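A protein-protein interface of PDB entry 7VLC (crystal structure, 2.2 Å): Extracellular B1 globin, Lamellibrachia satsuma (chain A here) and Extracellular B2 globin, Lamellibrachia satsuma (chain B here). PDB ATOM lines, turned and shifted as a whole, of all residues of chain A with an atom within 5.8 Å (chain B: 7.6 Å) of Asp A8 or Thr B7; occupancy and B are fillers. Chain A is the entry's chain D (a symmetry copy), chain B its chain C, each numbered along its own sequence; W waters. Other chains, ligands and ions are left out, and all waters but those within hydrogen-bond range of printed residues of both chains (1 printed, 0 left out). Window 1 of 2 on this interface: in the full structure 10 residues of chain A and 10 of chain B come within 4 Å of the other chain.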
ATOM      1  N   CYS A   4     -30.189  18.803 -21.445  1.00  0.00           N
ATOM      2  CA  CYS A   4     -29.559  17.874 -22.373  1.00  0.00           C
ATOM      3  C   CYS A   4     -28.406  18.588 -23.066  1.00  0.00           C
ATOM      4  O   CYS A   4     -28.288  19.817 -23.019  1.00  0.00           O
ATOM      5  CB  CYS A   4     -30.561  17.297 -23.392  1.00  0.00           C
ATOM      6  SG  CYS A   4     -31.209  18.450 -24.627  1.00  0.00           S
ATOM      7  N   SER A   5     -27.548  17.796 -23.706  1.00  0.00           N
ATOM      8  CA  SER A   5     -26.320  18.310 -24.290  1.00  0.00           C
ATOM      9  C   SER A   5     -26.624  19.218 -25.482  1.00  0.00           C
ATOM     10  O   SER A   5     -27.730  19.236 -26.028  1.00  0.00           O
ATOM     11  CB  SER A   5     -25.411  17.160 -24.725  1.00  0.00           C
ATOM     12  OG  SER A   5     -25.882  16.565 -25.922  1.00  0.00           O
ATOM     13  N   GLU A   6     -25.605  19.978 -25.888  1.00  0.00           N
ATOM     14  CA  GLU A   6     -25.769  20.915 -26.996  1.00  0.00           C
ATOM     15  C   GLU A   6     -25.940  20.188 -28.325  1.00  0.00           C
ATOM     16  O   GLU A   6     -26.713  20.628 -29.184  1.00  0.00           O
ATOM     17  CB  GLU A   6     -24.574  21.863 -27.056  1.00  0.00           C
ATOM     18  CG  GLU A   6     -24.510  22.690 -28.328  1.00  0.00           C
ATOM     19  CD  GLU A   6     -23.338  23.646 -28.346  1.00  0.00           C
ATOM     20  OE1 GLU A   6     -23.225  24.462 -27.407  1.00  0.00           O
ATOM     21  OE2 GLU A   6     -22.524  23.572 -29.292  1.00  0.00           O
ATOM     22  N   ALA A   7     -25.217  19.085 -28.523  1.00  0.00           N
ATOM     23  CA  ALA A   7     -25.382  18.316 -29.750  1.00  0.00           C
ATOM     24  C   ALA A   7     -26.741  17.625 -29.794  1.00  0.00           C
ATOM     25  O   ALA A   7     -27.378  17.572 -30.851  1.00  0.00           O
ATOM     26  CB  ALA A   7     -24.256  17.293 -29.892  1.00  0.00           C
ATOM     27  N   ASP A   8     -27.196  17.082 -28.662  1.00  0.00           N
ATOM     28  CA  ASP A   8     -28.532  16.491 -28.616  1.00  0.00           C
ATOM     29  C   ASP A   8     -29.601  17.550 -28.854  1.00  0.00           C
ATOM     30  O   ASP A   8     -30.519  17.353 -29.658  1.00  0.00           O
ATOM     31  CB  ASP A   8     -28.763  15.797 -27.271  1.00  0.00           C
ATOM     32  CG  ASP A   8     -28.055  14.455 -27.172  1.00  0.00           C
ATOM     33  OD1 ASP A   8     -27.714  13.876 -28.226  1.00  0.00           O
ATOM     34  OD2 ASP A   8     -27.861  13.977 -26.035  1.00  0.00           O
ATOM     35  N   ALA A   9     -29.494  18.684 -28.156  1.00  0.00           N
ATOM     36  CA  ALA A   9     -30.452  19.768 -28.350  1.00  0.00           C
ATOM     37  C   ALA A   9     -30.451  20.246 -29.794  1.00  0.00           C
ATOM     38  O   ALA A   9     -31.513  20.540 -30.358  1.00  0.00           O
ATOM     39  CB  ALA A   9     -30.136  20.924 -27.401  1.00  0.00           C
ATOM     40  N   THR A  10     -29.270  20.315 -30.413  1.00  0.00           N
ATOM     41  CA  THR A  10     -29.190  20.715 -31.815  1.00  0.00           C
ATOM     42  C   THR A  10     -29.983  19.768 -32.708  1.00  0.00           C
ATOM     43  O   THR A  10     -30.676  20.210 -33.632  1.00  0.00           O
ATOM     44  CB  THR A  10     -27.727  20.779 -32.255  1.00  0.00           C
ATOM     45  OG1 THR A  10     -27.038  21.762 -31.468  1.00  0.00           O
ATOM     46  CG2 THR A  10     -27.620  21.150 -33.730  1.00  0.00           C
ATOM     47  N   ILE A  11     -29.913  18.463 -32.438  1.00  0.00           N
ATOM     48  CA  ILE A  11     -30.673  17.504 -33.236  1.00  0.00           C
ATOM     49  C   ILE A  11     -32.168  17.685 -33.009  1.00  0.00           C
ATOM     50  O   ILE A  11     -32.959  17.667 -33.961  1.00  0.00           O
ATOM     51  CB  ILE A  11     -30.229  16.066 -32.921  1.00  0.00           C
ATOM     52  CG1 ILE A  11     -28.756  15.867 -33.285  1.00  0.00           C
ATOM     53  CG2 ILE A  11     -31.111  15.064 -33.660  1.00  0.00           C
ATOM     54  CD1 ILE A  11     -28.250  14.475 -32.998  1.00  0.00           C
ATOM     55  N   VAL A  12     -32.579  17.865 -31.751  1.00  0.00           N
ATOM     56  CA  VAL A  12     -34.000  18.019 -31.441  1.00  0.00           C
ATOM     57  C   VAL A  12     -34.551  19.285 -32.081  1.00  0.00           C
ATOM     58  O   VAL A  12     -35.640  19.279 -32.666  1.00  0.00           O
ATOM     59  CB  VAL A  12     -34.218  18.015 -29.917  1.00  0.00           C
ATOM     60  CG1 VAL A  12     -35.691  18.249 -29.585  1.00  0.00           C
ATOM     61  CG2 VAL A  12     -33.737  16.707 -29.322  1.00  0.00           C
ATOM     62  N   ILE A  13     -33.802  20.386 -31.993  1.00  0.00           N
ATOM     63  CA  ILE A  13     -34.272  21.664 -32.518  1.00  0.00           C
ATOM     64  C   ILE A  13     -34.416  21.603 -34.032  1.00  0.00           C
ATOM     65  O   ILE A  13     -35.407  22.087 -34.593  1.00  0.00           O
ATOM     66  CB  ILE A  13     -33.327  22.798 -32.074  1.00  0.00           C
ATOM     67  CG1 ILE A  13     -33.436  23.001 -30.559  1.00  0.00           C
ATOM     68  CG2 ILE A  13     -33.644  24.090 -32.818  1.00  0.00           C
ATOM     69  CD1 ILE A  13     -32.432  23.966 -29.980  1.00  0.00           C
ATOM     70  N   LEU A  82     -33.423  24.983 -25.305  1.00  0.00           N
ATOM     71  CA  LEU A  82     -32.700  23.868 -24.702  1.00  0.00           C
ATOM     72  C   LEU A  82     -31.248  24.225 -24.404  1.00  0.00           C
ATOM     73  O   LEU A  82     -30.644  23.641 -23.498  1.00  0.00           O
ATOM     74  CB  LEU A  82     -32.768  22.643 -25.614  1.00  0.00           C
ATOM     75  CG  LEU A  82     -34.060  21.822 -25.619  1.00  0.00           C
ATOM     76  CD1 LEU A  82     -34.029  20.790 -26.740  1.00  0.00           C
ATOM     77  CD2 LEU A  82     -34.281  21.146 -24.272  1.00  0.00           C
ATOM     78  N   ASN A 129     -34.765  10.896 -34.259  1.00  0.00           N
ATOM     79  CA  ASN A 129     -33.761  10.379 -33.341  1.00  0.00           C
ATOM     80  C   ASN A 129     -34.386  10.194 -31.966  1.00  0.00           C
ATOM     81  O   ASN A 129     -34.433  11.150 -31.179  1.00  0.00           O
ATOM     82  CB  ASN A 129     -32.562  11.328 -33.269  1.00  0.00           C
ATOM     83  CG  ASN A 129     -31.376  10.721 -32.538  1.00  0.00           C
ATOM     84  OD1 ASN A 129     -31.534  10.040 -31.524  1.00  0.00           O
ATOM     85  ND2 ASN A 129     -30.179  10.967 -33.056  1.00  0.00           N
ATOM     86  N   ASP A 131     -33.364   8.796 -29.216  1.00  0.00           N
ATOM     87  CA  ASP A 131     -32.483   8.967 -28.065  1.00  0.00           C
ATOM     88  C   ASP A 131     -32.212  10.441 -27.788  1.00  0.00           C
ATOM     89  O   ASP A 131     -32.285  10.886 -26.639  1.00  0.00           O
ATOM     90  CB  ASP A 131     -31.169   8.212 -28.284  1.00  0.00           C
ATOM     91  CG  ASP A 131     -31.327   6.712 -28.140  1.00  0.00           C
ATOM     92  OD1 ASP A 131     -32.444   6.251 -27.817  1.00  0.00           O
ATOM     93  OD2 ASP A 131     -30.328   5.992 -28.347  1.00  0.00           O
ATOM     94  N   ALA A 132     -31.896  11.213 -28.829  1.00  0.00           N
ATOM     95  CA  ALA A 132     -31.724  12.650 -28.645  1.00  0.00           C
ATOM     96  C   ALA A 132     -33.006  13.291 -28.128  1.00  0.00           C
ATOM     97  O   ALA A 132     -32.963  14.211 -27.302  1.00  0.00           O
ATOM     98  CB  ALA A 132     -31.286  13.296 -29.960  1.00  0.00           C
ATOM     99  N   ASN A 135     -33.408  12.272 -24.457  1.00  0.00           N
ATOM    100  CA  ASN A 135     -32.450  12.963 -23.604  1.00  0.00           C
ATOM    101  C   ASN A 135     -32.879  14.396 -23.318  1.00  0.00           C
ATOM    102  O   ASN A 135     -32.510  14.954 -22.280  1.00  0.00           O
ATOM    103  CB  ASN A 135     -31.060  12.942 -24.248  1.00  0.00           C
ATOM    104  CG  ASN A 135     -30.472  11.539 -24.331  1.00  0.00           C
ATOM    105  OD1 ASN A 135     -30.927  10.619 -23.649  1.00  0.00           O
ATOM    106  ND2 ASN A 135     -29.450  11.376 -25.163  1.00  0.00           N
ATOM    107  N   CYS A 136     -33.654  15.005 -24.214  1.00  0.00           N
ATOM    108  CA  CYS A 136     -34.090  16.385 -24.042  1.00  0.00           C
ATOM    109  C   CYS A 136     -35.536  16.501 -23.573  1.00  0.00           C
ATOM    110  O   CYS A 136     -35.840  17.353 -22.736  1.00  0.00           O
ATOM    111  CB  CYS A 136     -33.908  17.172 -25.346  1.00  0.00           C
ATOM    112  SG  CYS A 136     -32.199  17.296 -25.981  1.00  0.00           S
ATOM    113  N   SER B   4     -26.864  10.304 -19.271  1.00  0.00           N
ATOM    114  CA  SER B   4     -27.380   9.864 -20.556  1.00  0.00           C
ATOM    115  C   SER B   4     -26.251   9.740 -21.572  1.00  0.00           C
ATOM    116  O   SER B   4     -25.262  10.477 -21.529  1.00  0.00           O
ATOM    117  CB  SER B   4     -28.436  10.842 -21.076  1.00  0.00           C
ATOM    118  OG  SER B   4     -29.464  11.031 -20.121  1.00  0.00           O
ATOM    119  N   CYS B   5     -26.408   8.795 -22.493  1.00  0.00           N
ATOM    120  CA  CYS B   5     -25.483   8.657 -23.614  1.00  0.00           C
ATOM    121  C   CYS B   5     -25.798   9.750 -24.624  1.00  0.00           C
ATOM    122  O   CYS B   5     -26.744   9.636 -25.403  1.00  0.00           O
ATOM    123  CB  CYS B   5     -25.594   7.272 -24.238  1.00  0.00           C
ATOM    124  SG  CYS B   5     -24.744   7.100 -25.823  1.00  0.00           S
ATOM    125  N   THR B   6     -24.997  10.813 -24.613  1.00  0.00           N
ATOM    126  CA  THR B   6     -25.230  11.964 -25.469  1.00  0.00           C
ATOM    127  C   THR B   6     -24.632  11.738 -26.855  1.00  0.00           C
ATOM    128  O   THR B   6     -23.873  10.794 -27.096  1.00  0.00           O
ATOM    129  CB  THR B   6     -24.634  13.228 -24.844  1.00  0.00           C
ATOM    130  OG1 THR B   6     -23.205  13.146 -24.860  1.00  0.00           O
ATOM    131  CG2 THR B   6     -25.107  13.389 -23.401  1.00  0.00           C
ATOM    132  N   THR B   7     -24.998  12.629 -27.782  1.00  0.00           N
ATOM    133  CA  THR B   7     -24.398  12.606 -29.110  1.00  0.00           C
ATOM    134  C   THR B   7     -22.882  12.750 -29.025  1.00  0.00           C
ATOM    135  O   THR B   7     -22.147  12.100 -29.776  1.00  0.00           O
ATOM    136  CB  THR B   7     -24.994  13.719 -29.976  1.00  0.00           C
ATOM    137  OG1 THR B   7     -26.401  13.492 -30.161  1.00  0.00           O
ATOM    138  CG2 THR B   7     -24.308  13.774 -31.332  1.00  0.00           C
ATOM    139  N   GLU B   8     -22.398  13.592 -28.106  1.00  0.00           N
ATOM    140  CA  GLU B   8     -20.957  13.730 -27.904  1.00  0.00           C
ATOM    141  C   GLU B   8     -20.340  12.413 -27.455  1.00  0.00           C
ATOM    142  O   GLU B   8     -19.319  11.976 -27.996  1.00  0.00           O
ATOM    143  CB  GLU B   8     -20.666  14.831 -26.880  1.00  0.00           C
ATOM    144  CG  GLU B   8     -21.014  16.240 -27.338  1.00  0.00           C
ATOM    145  CD  GLU B   8     -22.463  16.627 -27.063  1.00  0.00           C
ATOM    146  OE1 GLU B   8     -23.286  15.740 -26.750  1.00  0.00           O
ATOM    147  OE2 GLU B   8     -22.776  17.833 -27.162  1.00  0.00           O
ATOM    148  N   ASP B   9     -20.948  11.768 -26.455  1.00  0.00           N
ATOM    149  CA  ASP B   9     -20.452  10.478 -25.988  1.00  0.00           C
ATOM    150  C   ASP B   9     -20.524   9.417 -27.078  1.00  0.00           C
ATOM    151  O   ASP B   9     -19.677   8.519 -27.127  1.00  0.00           O
ATOM    152  CB  ASP B   9     -21.240  10.028 -24.760  1.00  0.00           C
ATOM    153  CG  ASP B   9     -21.137  11.005 -23.607  1.00  0.00           C
ATOM    154  OD1 ASP B   9     -20.151  11.773 -23.559  1.00  0.00           O
ATOM    155  OD2 ASP B   9     -22.044  10.994 -22.745  1.00  0.00           O
ATOM    156  N   ARG B  10     -21.529   9.491 -27.951  1.00  0.00           N
ATOM    157  CA  ARG B  10     -21.613   8.536 -29.050  1.00  0.00           C
ATOM    158  C   ARG B  10     -20.419   8.672 -29.988  1.00  0.00           C
ATOM    159  O   ARG B  10     -19.817   7.665 -30.381  1.00  0.00           O
ATOM    160  CB  ARG B  10     -22.928   8.720 -29.806  1.00  0.00           C
ATOM    161  CG  ARG B  10     -24.116   8.090 -29.101  1.00  0.00           C
ATOM    162  CD  ARG B  10     -25.401   8.896 -29.283  1.00  0.00           C
ATOM    163  NE  ARG B  10     -26.301   8.695 -28.148  1.00  0.00           N
ATOM    164  CZ  ARG B  10     -27.326   7.848 -28.137  1.00  0.00           C
ATOM    165  NH1 ARG B  10     -27.608   7.125 -29.213  1.00  0.00           N
ATOM    166  NH2 ARG B  10     -28.075   7.731 -27.046  1.00  0.00           N
ATOM    167  N   ARG B  11     -20.059   9.910 -30.347  1.00  0.00           N
ATOM    168  CA  ARG B  11     -18.875  10.128 -31.176  1.00  0.00           C
ATOM    169  C   ARG B  11     -17.615   9.622 -30.481  1.00  0.00           C
ATOM    170  O   ARG B  11     -16.758   8.995 -31.116  1.00  0.00           O
ATOM    171  CB  ARG B  11     -18.726  11.614 -31.515  1.00  0.00           C
ATOM    172  CG  ARG B  11     -19.968  12.269 -32.118  1.00  0.00           C
ATOM    173  CD  ARG B  11     -19.719  13.746 -32.416  1.00  0.00           C
ATOM    174  NE  ARG B  11     -20.957  14.501 -32.625  1.00  0.00           N
ATOM    175  CZ  ARG B  11     -21.555  14.658 -33.802  1.00  0.00           C
ATOM    176  NH1 ARG B  11     -22.674  15.365 -33.888  1.00  0.00           N
ATOM    177  NH2 ARG B  11     -21.039  14.107 -34.892  1.00  0.00           N
ATOM    178  N   GLU B  12     -17.484   9.882 -29.174  1.00  0.00           N
ATOM    179  CA  GLU B  12     -16.283   9.456 -28.462  1.00  0.00           C
ATOM    180  C   GLU B  12     -16.181   7.939 -28.412  1.00  0.00           C
ATOM    181  O   GLU B  12     -15.084   7.382 -28.546  1.00  0.00           O
ATOM    182  CB  GLU B  12     -16.263  10.031 -27.050  1.00  0.00           C
ATOM    183  CG  GLU B  12     -15.728  11.444 -26.946  1.00  0.00           C
ATOM    184  CD  GLU B  12     -15.618  11.907 -25.504  1.00  0.00           C
ATOM    185  OE1 GLU B  12     -14.896  11.253 -24.724  1.00  0.00           O
ATOM    186  OE2 GLU B  12     -16.266  12.915 -25.148  1.00  0.00           O
ATOM    187  N   MET B  13     -17.308   7.253 -28.219  1.00  0.00           N
ATOM    188  CA  MET B  13     -17.265   5.796 -28.148  1.00  0.00           C
ATOM    189  C   MET B  13     -16.891   5.194 -29.494  1.00  0.00           C
ATOM    190  O   MET B  13     -16.096   4.250 -29.557  1.00  0.00           O
ATOM    191  CB  MET B  13     -18.604   5.240 -27.669  1.00  0.00           C
ATOM    192  CG  MET B  13     -18.529   3.774 -27.271  1.00  0.00           C
ATOM    193  SD  MET B  13     -20.117   3.116 -26.739  1.00  0.00           S
ATOM    194  CE  MET B  13     -19.649   1.514 -26.084  1.00  0.00           C
ATOM    195  N   GLN B  14     -17.446   5.732 -30.584  1.00  0.00           N
ATOM    196  CA  GLN B  14     -17.073   5.241 -31.904  1.00  0.00           C
ATOM    197  C   GLN B  14     -15.613   5.544 -32.219  1.00  0.00           C
ATOM    198  O   GLN B  14     -14.981   4.804 -32.982  1.00  0.00           O
ATOM    199  CB  GLN B  14     -17.995   5.839 -32.963  1.00  0.00           C
ATOM    200  CG  GLN B  14     -19.420   5.302 -32.904  1.00  0.00           C
ATOM    201  CD  GLN B  14     -20.410   6.182 -33.642  1.00  0.00           C
ATOM    202  OE1 GLN B  14     -20.126   7.345 -33.930  1.00  0.00           O
ATOM    203  NE2 GLN B  14     -21.578   5.633 -33.951  1.00  0.00           N
ATOM    204  N   LEU B  82     -25.453   3.558 -32.854  1.00  0.00           N
ATOM    205  CA  LEU B  82     -25.699   4.675 -31.950  1.00  0.00           C
ATOM    206  C   LEU B  82     -25.998   5.959 -32.716  1.00  0.00           C
ATOM    207  O   LEU B  82     -26.676   6.846 -32.189  1.00  0.00           O
ATOM    208  CB  LEU B  82     -24.505   4.876 -31.022  1.00  0.00           C
ATOM    209  CG  LEU B  82     -24.308   3.840 -29.911  1.00  0.00           C
ATOM    210  CD1 LEU B  82     -22.947   4.000 -29.253  1.00  0.00           C
ATOM    211  CD2 LEU B  82     -25.414   3.969 -28.878  1.00  0.00           C
ATOM    212  N   SER B  83     -25.520   6.068 -33.957  1.00  0.00           N
ATOM    213  CA  SER B  83     -25.833   7.208 -34.805  1.00  0.00           C
ATOM    214  C   SER B  83     -27.238   7.137 -35.389  1.00  0.00           C
ATOM    215  O   SER B  83     -27.744   8.158 -35.863  1.00  0.00           O
ATOM    216  CB  SER B  83     -24.818   7.303 -35.942  1.00  0.00           C
ATOM    217  OG  SER B  83     -23.493   7.314 -35.443  1.00  0.00           O
ATOM    218  N   CYS B 136     -22.630   5.136 -22.697  1.00  0.00           N
ATOM    219  CA  CYS B 136     -23.239   4.577 -23.897  1.00  0.00           C
ATOM    220  C   CYS B 136     -23.221   3.056 -23.908  1.00  0.00           C
ATOM    221  O   CYS B 136     -24.122   2.440 -24.490  1.00  0.00           O
ATOM    222  CB  CYS B 136     -22.545   5.131 -25.144  1.00  0.00           C
ATOM    223  SG  CYS B 136     -22.774   6.911 -25.348  1.00  0.00           S
HETATM  224  O   HOH W   1     -28.286  11.214 -28.273  1.00  0.00           O
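Printed residues of chain B that touch a printed residue of chain A: Ser B4, Cys B5, Thr B6, Thr B7, Glu B8 and Arg B10.
Of the 16 printed residues of chain A, 7 touch a printed residue of chain B.
Hydrophobic or aromatic side chains of chain A within 4 Å of the printed part of chain B: Ala A7 and Ile A11.
Along chain A the printed residues that touch a printed residue of chain B span positions 5 to 135.
Among the printed residues, Asp or Glu carboxylates within 4 Å of a Lys or Arg side-chain nitrogen of the other chain: Asp A131 with Arg B10 (3.1 Å).
The side-chain hydroxyl of Thr B6 sits at hydrogen-bond distance from the side-chain carboxylate of Glu B8, at 3.2 Å.
The side-chain hydroxyl (OG1) of Thr B6 lies within hydrogen-bond range of the backbone NH (N) of Asp B9 (3.1 Å).
O of Thr B6 lies close to NE of Arg B10, at 3.4 Å.
The guanidinium group (NH1) of Arg B10 sits at hydrogen-bond distance from the backbone carbonyl oxygen (O) of Leu B82 (3.1 Å).
O of Glu A6 lies within hydrogen-bond range of OG1 of Thr A10 (2.6 Å).
The backbone carbonyl oxygen (O) of Asp A131 lies close to the side-chain amide nitrogen (ND2) of Asn A135 (3.2 Å).
Among the printed residues, pairs that only touch across the chains: Asp A8 with Thr B6 (3.4 Å), Ile A11 with Thr B7 (3.5 Å), Asn A135 with Ser B4 (3.6 Å), Ala A7 with Thr B7 (3.7 Å), Ser A5 with Thr B6 (3.7 Å) and Glu A6 with Glu B8 (3.8 Å).
O of Cys B5 is in hydrogen-bond range of ND2 of Asn A135.
The backbone NH (N) of Thr B7 is in hydrogen-bond range of the side-chain carboxylate (OD1) of Asp A8 (3.0 Å).
The side-chain hydroxyl (OG) of Ser A5 is in hydrogen-bond range of the side-chain carboxylate (OE1) of Glu B8 (2.8 Å).
The side-chain carboxylate (OE2) of Glu B8 lies within hydrogen-bond range of the backbone NH (N) of Ala A7, 3.1 Å away.
The guanidinium group (NH1) of Arg B10 is in salt-bridge range of the side-chain carboxylate (OD2) of Asp A131.
Cys A4 touches none of the printed residues of chain B.
Printed residues of chain B within 4 Å of Glu A6: Glu B8.
Of chain B, only Thr B7 and Glu B8 come within 4 Å of Ala A7.
Of chain B, only Thr B6 (3.4 Å) and Thr B7 (2.4 Å) come within 4 Å of Asp A8.
Ala A9 touches none of the printed residues of chain B.
Of the printed residues of chain B, Asp A131 touches Arg B10 (3.1 Å).
Printed residues of chain B within 4 Å of Asn A135: Ser B4 (3.6 Å) and Cys B5 (3.2 Å).
Of the printed residues of chain A, Thr B6 touches Ser A5 (3.7 Å) and Asp A8 (3.4 Å).
Of chain A, only Ala A7 (3.7 Å), Asp A8 (2.4 Å) and Ile A11 (3.5 Å) come within 4 Å of Thr B7.
Printed residues of chain A within 4 Å of Glu B8: Ser A5, Glu A6 and Ala A7.
The nearest printed residue of chain B that does not touch Asp A8 is Cys B5 (4.5 Å).
The nearest residue of chain A that does not touch Thr B7 is Ser A5 (4.4 Å).
The nearest printed residue of chain B that does not touch Ile A11 is Arg B11 (5.7 Å).
Water W1 lies within hydrogen-bond range of OD1 of Asp A8 (2.7 Å), NE of Arg B10 (3.2 Å) and ND2 of Asn A135 (3.3 Å).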
